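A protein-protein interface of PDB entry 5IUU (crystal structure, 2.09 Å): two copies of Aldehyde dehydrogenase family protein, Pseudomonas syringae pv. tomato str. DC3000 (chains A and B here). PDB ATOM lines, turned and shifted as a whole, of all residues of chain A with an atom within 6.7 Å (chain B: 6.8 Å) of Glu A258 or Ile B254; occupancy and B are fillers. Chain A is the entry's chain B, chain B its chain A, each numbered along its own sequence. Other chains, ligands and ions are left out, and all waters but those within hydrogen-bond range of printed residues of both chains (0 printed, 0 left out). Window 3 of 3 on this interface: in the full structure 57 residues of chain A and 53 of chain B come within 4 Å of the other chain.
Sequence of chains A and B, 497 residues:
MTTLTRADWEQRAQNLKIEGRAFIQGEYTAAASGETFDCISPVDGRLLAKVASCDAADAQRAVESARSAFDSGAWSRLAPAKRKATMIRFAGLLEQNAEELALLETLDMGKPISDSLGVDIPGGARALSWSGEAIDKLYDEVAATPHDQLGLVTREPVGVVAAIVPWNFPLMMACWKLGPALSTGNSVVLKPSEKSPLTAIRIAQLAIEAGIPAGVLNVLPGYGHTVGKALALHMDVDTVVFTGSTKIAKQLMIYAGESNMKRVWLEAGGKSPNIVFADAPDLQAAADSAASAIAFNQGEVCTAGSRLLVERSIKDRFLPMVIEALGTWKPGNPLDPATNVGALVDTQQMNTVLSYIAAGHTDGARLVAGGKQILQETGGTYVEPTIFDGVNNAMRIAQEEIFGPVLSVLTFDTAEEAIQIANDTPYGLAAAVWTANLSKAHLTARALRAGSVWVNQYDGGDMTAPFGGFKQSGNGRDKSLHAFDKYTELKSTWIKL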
ATOM      1  N   LEU A 233      23.825  17.001 -18.125  1.00  0.00           N
ATOM      2  CA  LEU A 233      24.142  16.945 -16.703  1.00  0.00           C
ATOM      3  C   LEU A 233      23.906  18.263 -15.977  1.00  0.00           C
ATOM      4  O   LEU A 233      24.109  18.318 -14.758  1.00  0.00           O
ATOM      5  CB  LEU A 233      25.603  16.515 -16.505  1.00  0.00           C
ATOM      6  CG  LEU A 233      25.890  15.033 -16.745  1.00  0.00           C
ATOM      7  CD1 LEU A 233      27.384  14.769 -16.854  1.00  0.00           C
ATOM      8  CD2 LEU A 233      25.285  14.223 -15.598  1.00  0.00           C
ATOM      9  N   MET A 235      22.572  21.360 -13.917  1.00  0.00           N
ATOM     10  CA  MET A 235      21.616  21.368 -12.817  1.00  0.00           C
ATOM     11  C   MET A 235      20.540  22.434 -12.965  1.00  0.00           C
ATOM     12  O   MET A 235      19.600  22.454 -12.161  1.00  0.00           O
ATOM     13  CB  MET A 235      22.345  21.554 -11.473  1.00  0.00           C
ATOM     14  CG  MET A 235      23.257  20.371 -11.085  1.00  0.00           C
ATOM     15  SD  MET A 235      22.395  18.807 -10.706  1.00  0.00           S
ATOM     16  CE  MET A 235      21.390  19.335  -9.325  1.00  0.00           C
ATOM     17  N   LYS A 250      19.734   6.497 -24.168  1.00  0.00           N
ATOM     18  CA  LYS A 250      19.784   5.872 -22.848  1.00  0.00           C
ATOM     19  C   LYS A 250      20.736   6.609 -21.917  1.00  0.00           C
ATOM     20  O   LYS A 250      20.470   6.718 -20.707  1.00  0.00           O
ATOM     21  CB  LYS A 250      20.208   4.409 -22.967  1.00  0.00           C
ATOM     22  CG  LYS A 250      19.167   3.518 -23.602  1.00  0.00           C
ATOM     23  CD  LYS A 250      19.656   2.086 -23.659  1.00  0.00           C
ATOM     24  CE  LYS A 250      18.590   1.168 -24.237  1.00  0.00           C
ATOM     25  NZ  LYS A 250      19.131  -0.212 -24.415  1.00  0.00           N
ATOM     26  N   GLN A 251      21.865   7.098 -22.454  1.00  0.00           N
ATOM     27  CA  GLN A 251      22.812   7.832 -21.619  1.00  0.00           C
ATOM     28  C   GLN A 251      22.187   9.095 -21.047  1.00  0.00           C
ATOM     29  O   GLN A 251      22.495   9.473 -19.911  1.00  0.00           O
ATOM     30  CB  GLN A 251      24.076   8.188 -22.413  1.00  0.00           C
ATOM     31  CG  GLN A 251      25.244   7.236 -22.235  1.00  0.00           C
ATOM     32  CD  GLN A 251      25.659   7.066 -20.772  1.00  0.00           C
ATOM     33  OE1 GLN A 251      25.808   8.043 -20.028  1.00  0.00           O
ATOM     34  NE2 GLN A 251      25.838   5.819 -20.357  1.00  0.00           N
ATOM     35  N   MET A 253      19.005   9.628 -20.155  1.00  0.00           N
ATOM     36  CA  MET A 253      18.237   9.262 -18.963  1.00  0.00           C
ATOM     37  C   MET A 253      19.145   9.101 -17.751  1.00  0.00           C
ATOM     38  O   MET A 253      18.832   9.588 -16.656  1.00  0.00           O
ATOM     39  CB  MET A 253      17.448   7.977 -19.211  1.00  0.00           C
ATOM     40  CG  MET A 253      16.527   8.064 -20.413  1.00  0.00           C
ATOM     41  SD  MET A 253      15.219   6.816 -20.443  1.00  0.00           S
ATOM     42  CE  MET A 253      14.198   7.413 -19.072  1.00  0.00           C
ATOM     43  N   ILE A 254      20.294   8.450 -17.939  1.00  0.00           N
ATOM     44  CA  ILE A 254      21.241   8.275 -16.840  1.00  0.00           C
ATOM     45  C   ILE A 254      21.745   9.628 -16.352  1.00  0.00           C
ATOM     46  O   ILE A 254      21.726   9.915 -15.147  1.00  0.00           O
ATOM     47  CB  ILE A 254      22.398   7.355 -17.271  1.00  0.00           C
ATOM     48  CG1 ILE A 254      21.886   5.915 -17.443  1.00  0.00           C
ATOM     49  CG2 ILE A 254      23.543   7.450 -16.277  1.00  0.00           C
ATOM     50  CD1 ILE A 254      22.842   4.971 -18.174  1.00  0.00           C
ATOM     51  N   TYR A 255      22.187  10.492 -17.284  1.00  0.00           N
ATOM     52  CA  TYR A 255      22.650  11.826 -16.900  1.00  0.00           C
ATOM     53  C   TYR A 255      21.567  12.604 -16.163  1.00  0.00           C
ATOM     54  O   TYR A 255      21.864  13.355 -15.225  1.00  0.00           O
ATOM     55  CB  TYR A 255      23.091  12.636 -18.132  1.00  0.00           C
ATOM     56  CG  TYR A 255      24.331  12.153 -18.866  1.00  0.00           C
ATOM     57  CD1 TYR A 255      25.365  11.490 -18.201  1.00  0.00           C
ATOM     58  CD2 TYR A 255      24.469  12.388 -20.233  1.00  0.00           C
ATOM     59  CE1 TYR A 255      26.496  11.065 -18.886  1.00  0.00           C
ATOM     60  CE2 TYR A 255      25.582  11.975 -20.921  1.00  0.00           C
ATOM     61  CZ  TYR A 255      26.598  11.318 -20.252  1.00  0.00           C
ATOM     62  OH  TYR A 255      27.697  10.912 -20.970  1.00  0.00           O
ATOM     63  N   ALA A 256      20.309  12.488 -16.606  1.00  0.00           N
ATOM     64  CA  ALA A 256      19.236  13.179 -15.890  1.00  0.00           C
ATOM     65  C   ALA A 256      19.118  12.670 -14.456  1.00  0.00           C
ATOM     66  O   ALA A 256      18.999  13.465 -13.513  1.00  0.00           O
ATOM     67  CB  ALA A 256      17.903  13.006 -16.616  1.00  0.00           C
ATOM     68  N   GLY A 257      19.156  11.350 -14.275  1.00  0.00           N
ATOM     69  CA  GLY A 257      19.089  10.794 -12.930  1.00  0.00           C
ATOM     70  C   GLY A 257      20.290  11.162 -12.079  1.00  0.00           C
ATOM     71  O   GLY A 257      20.160  11.343 -10.865  1.00  0.00           O
ATOM     72  N   GLU A 258      21.466  11.311 -12.698  1.00  0.00           N
ATOM     73  CA  GLU A 258      22.658  11.713 -11.964  1.00  0.00           C
ATOM     74  C   GLU A 258      22.685  13.194 -11.627  1.00  0.00           C
ATOM     75  O   GLU A 258      23.542  13.609 -10.839  1.00  0.00           O
ATOM     76  CB  GLU A 258      23.920  11.351 -12.758  1.00  0.00           C
ATOM     77  CG  GLU A 258      24.100   9.848 -12.929  1.00  0.00           C
ATOM     78  CD  GLU A 258      25.315   9.475 -13.758  1.00  0.00           C
ATOM     79  OE1 GLU A 258      25.818  10.339 -14.513  1.00  0.00           O
ATOM     80  OE2 GLU A 258      25.762   8.307 -13.656  1.00  0.00           O
ATOM     81  N   SER A 259      21.773  14.006 -12.178  1.00  0.00           N
ATOM     82  CA  SER A 259      21.882  15.442 -12.022  1.00  0.00           C
ATOM     83  C   SER A 259      20.616  15.973 -11.323  1.00  0.00           C
ATOM     84  O   SER A 259      20.549  15.943 -10.093  1.00  0.00           O
ATOM     85  CB  SER A 259      22.158  16.146 -13.364  1.00  0.00           C
ATOM     86  OG  SER A 259      21.302  15.712 -14.410  1.00  0.00           O
ATOM     87  N   ASN A 260      19.646  16.504 -12.067  1.00  0.00           N
ATOM     88  CA  ASN A 260      18.549  17.254 -11.460  1.00  0.00           C
ATOM     89  C   ASN A 260      17.175  16.684 -11.801  1.00  0.00           C
ATOM     90  O   ASN A 260      16.173  17.375 -11.626  1.00  0.00           O
ATOM     91  CB  ASN A 260      18.618  18.727 -11.873  1.00  0.00           C
ATOM     92  CG  ASN A 260      18.319  18.933 -13.355  1.00  0.00           C
ATOM     93  OD1 ASN A 260      18.393  17.994 -14.147  1.00  0.00           O
ATOM     94  ND2 ASN A 260      17.992  20.165 -13.731  1.00  0.00           N
ATOM     95  N   MET A 261      17.106  15.450 -12.292  1.00  0.00           N
ATOM     96  CA  MET A 261      15.832  14.820 -12.636  1.00  0.00           C
ATOM     97  C   MET A 261      15.118  15.572 -13.764  1.00  0.00           C
ATOM     98  O   MET A 261      13.888  15.542 -13.861  1.00  0.00           O
ATOM     99  CB  MET A 261      14.920  14.705 -11.398  1.00  0.00           C
ATOM    100  CG  MET A 261      13.972  13.519 -11.373  1.00  0.00           C
ATOM    101  SD  MET A 261      12.758  13.657 -10.004  1.00  0.00           S
ATOM    102  CE  MET A 261      13.883  13.684  -8.638  1.00  0.00           C
ATOM    103  N   ALA B 232      12.040  -1.865 -12.193  1.00  0.00           N
ATOM    104  CA  ALA B 232      12.591  -0.684 -12.853  1.00  0.00           C
ATOM    105  C   ALA B 232      13.635  -1.054 -13.894  1.00  0.00           C
ATOM    106  O   ALA B 232      13.824  -0.322 -14.884  1.00  0.00           O
ATOM    107  CB  ALA B 232      13.199   0.251 -11.810  1.00  0.00           C
ATOM    108  N   LEU B 233      14.328  -2.170 -13.683  1.00  0.00           N
ATOM    109  CA  LEU B 233      15.336  -2.683 -14.597  1.00  0.00           C
ATOM    110  C   LEU B 233      14.781  -3.682 -15.595  1.00  0.00           C
ATOM    111  O   LEU B 233      15.519  -4.125 -16.474  1.00  0.00           O
ATOM    112  CB  LEU B 233      16.468  -3.341 -13.806  1.00  0.00           C
ATOM    113  CG  LEU B 233      17.396  -2.364 -13.093  1.00  0.00           C
ATOM    114  CD1 LEU B 233      18.262  -3.112 -12.080  1.00  0.00           C
ATOM    115  CD2 LEU B 233      18.264  -1.647 -14.145  1.00  0.00           C
ATOM    116  N   ALA B 249      13.424   8.512  -7.088  1.00  0.00           N
ATOM    117  CA  ALA B 249      12.971   8.974  -8.400  1.00  0.00           C
ATOM    118  C   ALA B 249      14.138   9.089  -9.381  1.00  0.00           C
ATOM    119  O   ALA B 249      14.071   8.586 -10.510  1.00  0.00           O
ATOM    120  CB  ALA B 249      12.251  10.320  -8.269  1.00  0.00           C
ATOM    121  N   LYS B 250      15.235   9.721  -8.949  1.00  0.00           N
ATOM    122  CA  LYS B 250      16.420   9.826  -9.808  1.00  0.00           C
ATOM    123  C   LYS B 250      16.996   8.456 -10.140  1.00  0.00           C
ATOM    124  O   LYS B 250      17.428   8.213 -11.277  1.00  0.00           O
ATOM    125  CB  LYS B 250      17.486  10.683  -9.132  1.00  0.00           C
ATOM    126  CG  LYS B 250      17.111  12.144  -9.009  1.00  0.00           C
ATOM    127  CD  LYS B 250      18.242  12.908  -8.362  1.00  0.00           C
ATOM    128  CE  LYS B 250      17.819  14.300  -7.985  1.00  0.00           C
ATOM    129  NZ  LYS B 250      18.921  15.024  -7.331  1.00  0.00           N
ATOM    130  N   GLN B 251      17.012   7.543  -9.156  1.00  0.00           N
ATOM    131  CA  GLN B 251      17.531   6.199  -9.399  1.00  0.00           C
ATOM    132  C   GLN B 251      16.757   5.495 -10.506  1.00  0.00           C
ATOM    133  O   GLN B 251      17.336   4.737 -11.293  1.00  0.00           O
ATOM    134  CB  GLN B 251      17.475   5.365  -8.113  1.00  0.00           C
ATOM    135  CG  GLN B 251      18.816   5.173  -7.410  1.00  0.00           C
ATOM    136  CD  GLN B 251      19.940   4.723  -8.343  1.00  0.00           C
ATOM    137  OE1 GLN B 251      19.737   3.930  -9.275  1.00  0.00           O
ATOM    138  NE2 GLN B 251      21.140   5.237  -8.096  1.00  0.00           N
ATOM    139  N   LEU B 252      15.444   5.731 -10.582  1.00  0.00           N
ATOM    140  CA  LEU B 252      14.633   5.043 -11.582  1.00  0.00           C
ATOM    141  C   LEU B 252      14.981   5.500 -12.997  1.00  0.00           C
ATOM    142  O   LEU B 252      14.954   4.697 -13.938  1.00  0.00           O
ATOM    143  CB  LEU B 252      13.145   5.268 -11.291  1.00  0.00           C
ATOM    144  CG  LEU B 252      12.625   4.661  -9.988  1.00  0.00           C
ATOM    145  CD1 LEU B 252      11.141   4.908  -9.856  1.00  0.00           C
ATOM    146  CD2 LEU B 252      12.923   3.186  -9.942  1.00  0.00           C
ATOM    147  N   MET B 253      15.287   6.789 -13.172  1.00  0.00           N
ATOM    148  CA  MET B 253      15.770   7.247 -14.470  1.00  0.00           C
ATOM    149  C   MET B 253      17.046   6.516 -14.846  1.00  0.00           C
ATOM    150  O   MET B 253      17.214   6.075 -15.992  1.00  0.00           O
ATOM    151  CB  MET B 253      15.989   8.761 -14.445  1.00  0.00           C
ATOM    152  CG  MET B 253      14.684   9.518 -14.294  1.00  0.00           C
ATOM    153  SD  MET B 253      14.813  11.294 -14.550  1.00  0.00           S
ATOM    154  CE  MET B 253      14.809  11.354 -16.354  1.00  0.00           C
ATOM    155  N   ILE B 254      17.941   6.339 -13.874  1.00  0.00           N
ATOM    156  CA  ILE B 254      19.179   5.615 -14.131  1.00  0.00           C
ATOM    157  C   ILE B 254      18.878   4.172 -14.528  1.00  0.00           C
ATOM    158  O   ILE B 254      19.379   3.676 -15.547  1.00  0.00           O
ATOM    159  CB  ILE B 254      20.095   5.716 -12.902  1.00  0.00           C
ATOM    160  CG1 ILE B 254      20.426   7.198 -12.669  1.00  0.00           C
ATOM    161  CG2 ILE B 254      21.323   4.854 -13.080  1.00  0.00           C
ATOM    162  CD1 ILE B 254      21.287   7.479 -11.489  1.00  0.00           C
ATOM    163  N   TYR B 255      18.018   3.492 -13.754  1.00  0.00           N
ATOM    164  CA  TYR B 255      17.643   2.116 -14.091  1.00  0.00           C
ATOM    165  C   TYR B 255      17.017   2.028 -15.473  1.00  0.00           C
ATOM    166  O   TYR B 255      17.270   1.073 -16.218  1.00  0.00           O
ATOM    167  CB  TYR B 255      16.652   1.561 -13.061  1.00  0.00           C
ATOM    168  CG  TYR B 255      17.213   1.380 -11.677  1.00  0.00           C
ATOM    169  CD1 TYR B 255      18.539   1.021 -11.486  1.00  0.00           C
ATOM    170  CD2 TYR B 255      16.408   1.553 -10.558  1.00  0.00           C
ATOM    171  CE1 TYR B 255      19.046   0.841 -10.217  1.00  0.00           C
ATOM    172  CE2 TYR B 255      16.902   1.378  -9.291  1.00  0.00           C
ATOM    173  CZ  TYR B 255      18.221   1.026  -9.122  1.00  0.00           C
ATOM    174  OH  TYR B 255      18.720   0.861  -7.851  1.00  0.00           O
ATOM    175  N   ALA B 256      16.141   2.984 -15.805  1.00  0.00           N
ATOM    176  CA  ALA B 256      15.541   3.016 -17.138  1.00  0.00           C
ATOM    177  C   ALA B 256      16.608   3.100 -18.221  1.00  0.00           C
ATOM    178  O   ALA B 256      16.573   2.350 -19.209  1.00  0.00           O
ATOM    179  CB  ALA B 256      14.580   4.200 -17.257  1.00  0.00           C
ATOM    180  N   GLY B 257      17.560   4.021 -18.058  1.00  0.00           N
ATOM    181  CA  GLY B 257      18.612   4.167 -19.051  1.00  0.00           C
ATOM    182  C   GLY B 257      19.514   2.951 -19.142  1.00  0.00           C
ATOM    183  O   GLY B 257      19.985   2.604 -20.227  1.00  0.00           O
ATOM    184  N   GLU B 258      19.739   2.269 -18.019  1.00  0.00           N
ATOM    185  CA  GLU B 258      20.570   1.074 -18.022  1.00  0.00           C
ATOM    186  C   GLU B 258      19.869  -0.138 -18.614  1.00  0.00           C
ATOM    187  O   GLU B 258      20.536  -1.149 -18.870  1.00  0.00           O
ATOM    188  CB  GLU B 258      21.027   0.760 -16.596  1.00  0.00           C
ATOM    189  CG  GLU B 258      22.070   1.731 -16.071  1.00  0.00           C
ATOM    190  CD  GLU B 258      22.344   1.567 -14.589  1.00  0.00           C
ATOM    191  OE1 GLU B 258      21.638   0.766 -13.936  1.00  0.00           O
ATOM    192  OE2 GLU B 258      23.278   2.237 -14.083  1.00  0.00           O
ATOM    193  N   SER B 259      18.554  -0.074 -18.853  1.00  0.00           N
ATOM    194  CA  SER B 259      17.813  -1.260 -19.241  1.00  0.00           C
ATOM    195  C   SER B 259      17.231  -1.035 -20.621  1.00  0.00           C
ATOM    196  O   SER B 259      17.902  -1.305 -21.625  1.00  0.00           O
ATOM    197  CB  SER B 259      16.761  -1.635 -18.173  1.00  0.00           C
ATOM    198  OG  SER B 259      15.925  -0.539 -17.823  1.00  0.00           O
ATOM    199  N   VAL B 264       9.432   6.771 -17.773  1.00  0.00           N
ATOM    200  CA  VAL B 264       9.441   6.940 -16.323  1.00  0.00           C
ATOM    201  C   VAL B 264       8.641   8.186 -15.961  1.00  0.00           C
ATOM    202  O   VAL B 264       8.921   9.273 -16.467  1.00  0.00           O
ATOM    203  CB  VAL B 264      10.878   7.047 -15.775  1.00  0.00           C
ATOM    204  CG1 VAL B 264      10.855   7.161 -14.265  1.00  0.00           C
ATOM    205  CG2 VAL B 264      11.682   5.833 -16.184  1.00  0.00           C
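Printed residues of chain A that touch a printed residue of chain B: Lys A250, Met A253, Ile A254, Ala A256, Gly A257, Glu A258, Ser A259 and Met A261.
Hydrophobic or aromatic side chains of chain A within 4 Å of the printed part of chain B: Met A253, Ile A254, Ala A256 and Met A261.
Hydrophobic or aromatic side chains of chain B within 4 Å of the printed part of chain A: Ala B249, Met B253, Ile B254 and Ala B256.
Among the printed residues, no Asp or Glu carboxylate lies within 4 Å of a Lys or Arg side-chain nitrogen of the other chain.
Among the printed residues, merely in contact across the chains: Lys A250 with Gly B257 (3.3 Å), Met A253 with Met B253 (3.7 Å), Met A253 with Ala B256 (3.7 Å), Met A253 with Gly B257 (3.99 Å), Ile A254 with Ile B254 (3.9 Å), Ile A254 with Glu B258 (3.9 Å), Ala A256 with Met B253 (3.5 Å), Gly A257 with Lys B250 (3.3 Å), Gly A257 with Ile B254 (3.8 Å), Glu A258 with Ile B254 (3.9 Å), Met A261 with Ala B249 (3.8 Å), Met A261 with Lys B250 (3.6 Å) and Met A261 with Met B253 (3.97 Å).
Lys A250 touches Ser B259, and with the chains exchanged Ser A259 touches Lys B250.
Met B253 touches its own counterpart, Met A253.
Ile A254 touches Glu B258, and with the chains exchanged Glu A258 touches Ile B254.
Gly A257 touches Ile B254, but with the chains exchanged Ile A254 does not touch Gly B257 (4.01 Å).
Of the 15 pairs that touch across the chains among the printed residues, 10 have their exchanged pair printed and touching as well.
The backbone carbonyl oxygen of Ala A256 sits at hydrogen-bond distance from the backbone NH of Met A261 (3.0 Å).
The backbone carbonyl oxygen (O) of Tyr A255 is in hydrogen-bond range of the side-chain hydroxyl (OG) of Ser A259, 2.6 Å away.
The backbone carbonyl oxygen (O) of Ala B256 is in hydrogen-bond range of the side-chain hydroxyl (OG) of Ser B259 (3.3 Å).
O of Ala A256 lies within hydrogen-bond range of OG of Ser A259 (3.3 Å).
O of Tyr B255 lies within hydrogen-bond range of OG of Ser B259 (2.6 Å).
NZ of Lys A250 is in hydrogen-bond range of O of Ser B259, at 3.2 Å.
The side-chain amino group (NZ) of Lys B250 is in hydrogen-bond range of the backbone carbonyl oxygen (O) of Ser A259, 3.3 Å away.
Of the printed residues of chain B, Lys A250 touches Gly B257 and Ser B259.
Printed residues of chain B within 4 Å of Ala A256: Met B253.
Of chain B, only Ile B254 comes within 4 Å of Glu A258.
Of the printed residues of chain B, Ser A259 touches Lys B250 (3.3 Å).
Of the printed residues of chain A, Met B253 touches Met A253 (3.7 Å), Ala A256 (3.5 Å) and Met A261 (3.97 Å).
Of chain A, only Ile A254, Gly A257 and Glu A258 come within 4 Å of Ile B254.
Printed residues of chain A within 4 Å of Ala B256: Met A253.
The nearest residue of chain A that does not touch Ile B254 is Met A253 (4.4 Å).
The nearest printed residue of chain B that does not touch Met A253 is Val B264 (4.1 Å).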
